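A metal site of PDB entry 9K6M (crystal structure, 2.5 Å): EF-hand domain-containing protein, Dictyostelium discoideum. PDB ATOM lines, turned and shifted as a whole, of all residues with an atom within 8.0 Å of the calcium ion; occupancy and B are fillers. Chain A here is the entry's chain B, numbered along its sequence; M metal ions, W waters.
Water W1 lies within hydrogen-bond range of the side-chain carboxylate (OD2) of Asp 103 and the side-chain carboxylate (OD2) of Asp 105.
The side-chain carboxylate (OD1) of Asp 101 is bound to the calcium ion, 2.2 Å away.
O of Leu 107 is bound to the calcium ion.
The calcium ion is bound by the side-chain carboxylate (OD1) of Asp 103, at 2.3 Å.
OE1 of Glu 112 is bound to the calcium ion (2.4 Å).
OD1 of Asp 105 binds the calcium ion.
Water W1 binds the calcium ion (2.5 Å).
The side-chain carboxylate (OE2) of Glu 112 binds the calcium ion, 2.6 Å away.
The calcium ion has seven donor atoms within binding distance.
The side-chain carboxylate (OD1) of Asp 101 lies close to the backbone NH (N) of Gly 104 (3.2 Å).
The backbone NH (N) of Gly 106 sits at hydrogen-bond distance from the side-chain carboxylate (OD2) of Asp 101, 2.7 Å away.
N of Glu 112 lies close to OG of Ser 109, at 3.3 Å.
The side-chain carboxylate (OE2) of Glu 112 lies close to the backbone NH (N) of Val 102 (3.4 Å).
The nearest printed residue that does not touch the calcium ion is Ser 109 (4.2 Å).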
ATOM      1  N   LYS A  55      10.922  19.751 -18.946  1.00  0.00           N
ATOM      2  CA  LYS A  55      11.129  20.907 -19.775  1.00  0.00           C
ATOM      3  C   LYS A  55       9.939  20.967 -20.719  1.00  0.00           C
ATOM      4  O   LYS A  55       9.516  19.936 -21.236  1.00  0.00           O
ATOM      5  CB  LYS A  55      12.483  20.836 -20.490  1.00  0.00           C
ATOM      6  CG  LYS A  55      12.618  19.800 -21.584  1.00  0.00           C
ATOM      7  CD  LYS A  55      13.998  19.777 -22.199  1.00  0.00           C
ATOM      8  CE  LYS A  55      14.040  19.273 -23.631  1.00  0.00           C
ATOM      9  NZ  LYS A  55      13.323  20.167 -24.579  1.00  0.00           N
ATOM     10  N   PHE A  60      11.926  13.911 -19.716  1.00  0.00           N
ATOM     11  CA  PHE A  60      13.000  13.401 -20.533  1.00  0.00           C
ATOM     12  C   PHE A  60      14.048  12.705 -19.677  1.00  0.00           C
ATOM     13  O   PHE A  60      14.167  12.975 -18.479  1.00  0.00           O
ATOM     14  CB  PHE A  60      13.666  14.536 -21.310  1.00  0.00           C
ATOM     15  CG  PHE A  60      12.810  15.191 -22.363  1.00  0.00           C
ATOM     16  CD1 PHE A  60      11.822  16.096 -22.010  1.00  0.00           C
ATOM     17  CD2 PHE A  60      13.002  14.909 -23.703  1.00  0.00           C
ATOM     18  CE1 PHE A  60      11.031  16.675 -22.975  1.00  0.00           C
ATOM     19  CE2 PHE A  60      12.226  15.515 -24.676  1.00  0.00           C
ATOM     20  CZ  PHE A  60      11.235  16.395 -24.308  1.00  0.00           C
ATOM     21  N   MET A  61      14.804  11.786 -20.318  1.00  0.00           N
ATOM     22  CA  MET A  61      15.808  11.009 -19.635  1.00  0.00           C
ATOM     23  C   MET A  61      17.185  11.501 -20.049  1.00  0.00           C
ATOM     24  O   MET A  61      17.436  11.686 -21.224  1.00  0.00           O
ATOM     25  CB  MET A  61      15.744   9.541 -20.016  1.00  0.00           C
ATOM     26  CG  MET A  61      14.632   8.777 -19.415  1.00  0.00           C
ATOM     27  SD  MET A  61      14.539   7.113 -20.175  1.00  0.00           S
ATOM     28  CE  MET A  61      13.179   6.456 -19.211  1.00  0.00           C
ATOM     29  N   PHE A  97      22.182   4.428 -26.036  1.00  0.00           N
ATOM     30  CA  PHE A  97      21.611   5.760 -25.852  1.00  0.00           C
ATOM     31  C   PHE A  97      21.617   6.494 -27.188  1.00  0.00           C
ATOM     32  O   PHE A  97      20.660   7.174 -27.504  1.00  0.00           O
ATOM     33  CB  PHE A  97      22.345   6.555 -24.772  1.00  0.00           C
ATOM     34  CG  PHE A  97      21.760   7.911 -24.483  1.00  0.00           C
ATOM     35  CD1 PHE A  97      22.035   8.993 -25.304  1.00  0.00           C
ATOM     36  CD2 PHE A  97      20.934   8.100 -23.371  1.00  0.00           C
ATOM     37  CE1 PHE A  97      21.476  10.236 -25.036  1.00  0.00           C
ATOM     38  CE2 PHE A  97      20.368   9.340 -23.118  1.00  0.00           C
ATOM     39  CZ  PHE A  97      20.643  10.398 -23.946  1.00  0.00           C
ATOM     40  N   ALA A 100      18.751   5.277 -29.273  1.00  0.00           N
ATOM     41  CA  ALA A 100      17.487   5.769 -28.742  1.00  0.00           C
ATOM     42  C   ALA A 100      17.248   7.245 -29.050  1.00  0.00           C
ATOM     43  O   ALA A 100      16.095   7.608 -29.266  1.00  0.00           O
ATOM     44  CB  ALA A 100      17.420   5.516 -27.268  1.00  0.00           C
ATOM     45  N   ASP A 101      18.310   8.075 -29.094  1.00  0.00           N
ATOM     46  CA  ASP A 101      18.183   9.513 -29.292  1.00  0.00           C
ATOM     47  C   ASP A 101      18.141   9.820 -30.783  1.00  0.00           C
ATOM     48  O   ASP A 101      19.104  10.351 -31.368  1.00  0.00           O
ATOM     49  CB  ASP A 101      19.338  10.238 -28.621  1.00  0.00           C
ATOM     50  CG  ASP A 101      19.173  11.732 -28.547  1.00  0.00           C
ATOM     51  OD1 ASP A 101      18.014  12.197 -28.703  1.00  0.00           O
ATOM     52  OD2 ASP A 101      20.211  12.385 -28.320  1.00  0.00           O
ATOM     53  N   VAL A 102      16.994   9.546 -31.399  1.00  0.00           N
ATOM     54  CA  VAL A 102      16.819   9.744 -32.817  1.00  0.00           C
ATOM     55  C   VAL A 102      17.021  11.204 -33.202  1.00  0.00           C
ATOM     56  O   VAL A 102      17.608  11.451 -34.249  1.00  0.00           O
ATOM     57  CB  VAL A 102      15.451   9.195 -33.272  1.00  0.00           C
ATOM     58  CG1 VAL A 102      15.350   9.114 -34.780  1.00  0.00           C
ATOM     59  CG2 VAL A 102      15.222   7.828 -32.650  1.00  0.00           C
ATOM     60  N   ASP A 103      16.576  12.146 -32.346  1.00  0.00           N
ATOM     61  CA  ASP A 103      16.606  13.564 -32.671  1.00  0.00           C
ATOM     62  C   ASP A 103      17.959  14.186 -32.334  1.00  0.00           C
ATOM     63  O   ASP A 103      18.252  15.277 -32.792  1.00  0.00           O
ATOM     64  CB  ASP A 103      15.429  14.317 -32.023  1.00  0.00           C
ATOM     65  CG  ASP A 103      15.443  14.408 -30.510  1.00  0.00           C
ATOM     66  OD1 ASP A 103      16.404  13.909 -29.897  1.00  0.00           O
ATOM     67  OD2 ASP A 103      14.487  14.951 -29.948  1.00  0.00           O
ATOM     68  N   GLY A 104      18.813  13.503 -31.548  1.00  0.00           N
ATOM     69  CA  GLY A 104      20.150  13.987 -31.263  1.00  0.00           C
ATOM     70  C   GLY A 104      20.200  15.120 -30.245  1.00  0.00           C
ATOM     71  O   GLY A 104      21.233  15.775 -30.128  1.00  0.00           O
ATOM     72  N   ASP A 105      19.105  15.322 -29.484  1.00  0.00           N
ATOM     73  CA  ASP A 105      19.046  16.375 -28.491  1.00  0.00           C
ATOM     74  C   ASP A 105      19.801  15.992 -27.221  1.00  0.00           C
ATOM     75  O   ASP A 105      19.922  16.844 -26.329  1.00  0.00           O
ATOM     76  CB  ASP A 105      17.611  16.799 -28.190  1.00  0.00           C
ATOM     77  CG  ASP A 105      16.813  15.847 -27.316  1.00  0.00           C
ATOM     78  OD1 ASP A 105      17.306  14.704 -27.089  1.00  0.00           O
ATOM     79  OD2 ASP A 105      15.699  16.277 -26.872  1.00  0.00           O
ATOM     80  N   GLY A 106      20.326  14.759 -27.135  1.00  0.00           N
ATOM     81  CA  GLY A 106      21.128  14.334 -25.994  1.00  0.00           C
ATOM     82  C   GLY A 106      20.293  13.904 -24.787  1.00  0.00           C
ATOM     83  O   GLY A 106      20.835  13.651 -23.729  1.00  0.00           O
ATOM     84  N   LEU A 107      18.983  13.802 -24.978  1.00  0.00           N
ATOM     85  CA  LEU A 107      18.055  13.284 -23.986  1.00  0.00           C
ATOM     86  C   LEU A 107      17.127  12.267 -24.664  1.00  0.00           C
ATOM     87  O   LEU A 107      16.951  12.302 -25.885  1.00  0.00           O
ATOM     88  CB  LEU A 107      17.235  14.456 -23.457  1.00  0.00           C
ATOM     89  CG  LEU A 107      18.028  15.583 -22.799  1.00  0.00           C
ATOM     90  CD1 LEU A 107      17.097  16.747 -22.452  1.00  0.00           C
ATOM     91  CD2 LEU A 107      18.756  15.089 -21.558  1.00  0.00           C
ATOM     92  N   ILE A 108      16.491  11.407 -23.878  1.00  0.00           N
ATOM     93  CA  ILE A 108      15.556  10.442 -24.429  1.00  0.00           C
ATOM     94  C   ILE A 108      14.141  10.859 -24.103  1.00  0.00           C
ATOM     95  O   ILE A 108      13.781  10.908 -22.922  1.00  0.00           O
ATOM     96  CB  ILE A 108      15.828   9.026 -23.877  1.00  0.00           C
ATOM     97  CG1 ILE A 108      17.278   8.587 -24.096  1.00  0.00           C
ATOM     98  CG2 ILE A 108      14.847   8.044 -24.488  1.00  0.00           C
ATOM     99  CD1 ILE A 108      17.707   8.561 -25.559  1.00  0.00           C
ATOM    100  N   SER A 109      13.328  11.087 -25.151  1.00  0.00           N
ATOM    101  CA  SER A 109      11.913  11.425 -25.033  1.00  0.00           C
ATOM    102  C   SER A 109      11.079  10.169 -24.769  1.00  0.00           C
ATOM    103  O   SER A 109      11.556   9.047 -24.934  1.00  0.00           O
ATOM    104  CB  SER A 109      11.433  12.182 -26.285  1.00  0.00           C
ATOM    105  OG  SER A 109      11.366  11.349 -27.444  1.00  0.00           O
ATOM    106  N   PHE A 110       9.798  10.376 -24.415  1.00  0.00           N
ATOM    107  CA  PHE A 110       8.893   9.271 -24.106  1.00  0.00           C
ATOM    108  C   PHE A 110       8.749   8.355 -25.318  1.00  0.00           C
ATOM    109  O   PHE A 110       8.753   7.143 -25.144  1.00  0.00           O
ATOM    110  CB  PHE A 110       7.516   9.782 -23.646  1.00  0.00           C
ATOM    111  CG  PHE A 110       6.423   8.739 -23.661  1.00  0.00           C
ATOM    112  CD1 PHE A 110       6.318   7.786 -22.659  1.00  0.00           C
ATOM    113  CD2 PHE A 110       5.535   8.666 -24.729  1.00  0.00           C
ATOM    114  CE1 PHE A 110       5.329   6.814 -22.710  1.00  0.00           C
ATOM    115  CE2 PHE A 110       4.569   7.693 -24.790  1.00  0.00           C
ATOM    116  CZ  PHE A 110       4.452   6.771 -23.778  1.00  0.00           C
ATOM    117  N   GLU A 112      10.902   8.120 -27.934  1.00  0.00           N
ATOM    118  CA  GLU A 112      12.180   7.492 -28.158  1.00  0.00           C
ATOM    119  C   GLU A 112      12.322   6.254 -27.259  1.00  0.00           C
ATOM    120  O   GLU A 112      12.807   5.244 -27.748  1.00  0.00           O
ATOM    121  CB  GLU A 112      13.318   8.485 -27.940  1.00  0.00           C
ATOM    122  CG  GLU A 112      13.507   9.494 -29.069  1.00  0.00           C
ATOM    123  CD  GLU A 112      14.409  10.688 -28.737  1.00  0.00           C
ATOM    124  OE1 GLU A 112      14.751  10.881 -27.557  1.00  0.00           O
ATOM    125  OE2 GLU A 112      14.780  11.466 -29.665  1.00  0.00           O
ATOM    126  N   PHE A 113      11.905   6.336 -25.988  1.00  0.00           N
ATOM    127  CA  PHE A 113      12.132   5.272 -25.026  1.00  0.00           C
ATOM    128  C   PHE A 113      11.197   4.096 -25.275  1.00  0.00           C
ATOM    129  O   PHE A 113      11.599   2.951 -25.090  1.00  0.00           O
ATOM    130  CB  PHE A 113      11.918   5.736 -23.594  1.00  0.00           C
ATOM    131  CG  PHE A 113      12.049   4.671 -22.547  1.00  0.00           C
ATOM    132  CD1 PHE A 113      13.277   4.115 -22.248  1.00  0.00           C
ATOM    133  CD2 PHE A 113      10.928   4.198 -21.890  1.00  0.00           C
ATOM    134  CE1 PHE A 113      13.402   3.134 -21.280  1.00  0.00           C
ATOM    135  CE2 PHE A 113      11.061   3.230 -20.897  1.00  0.00           C
ATOM    136  CZ  PHE A 113      12.294   2.696 -20.600  1.00  0.00           C
HETATM  137 CA    CA M   1      16.023  12.847 -27.881  1.00  0.00          CA
HETATM  138  O   HOH W   1      13.969  14.171 -27.360  1.00  0.00           O
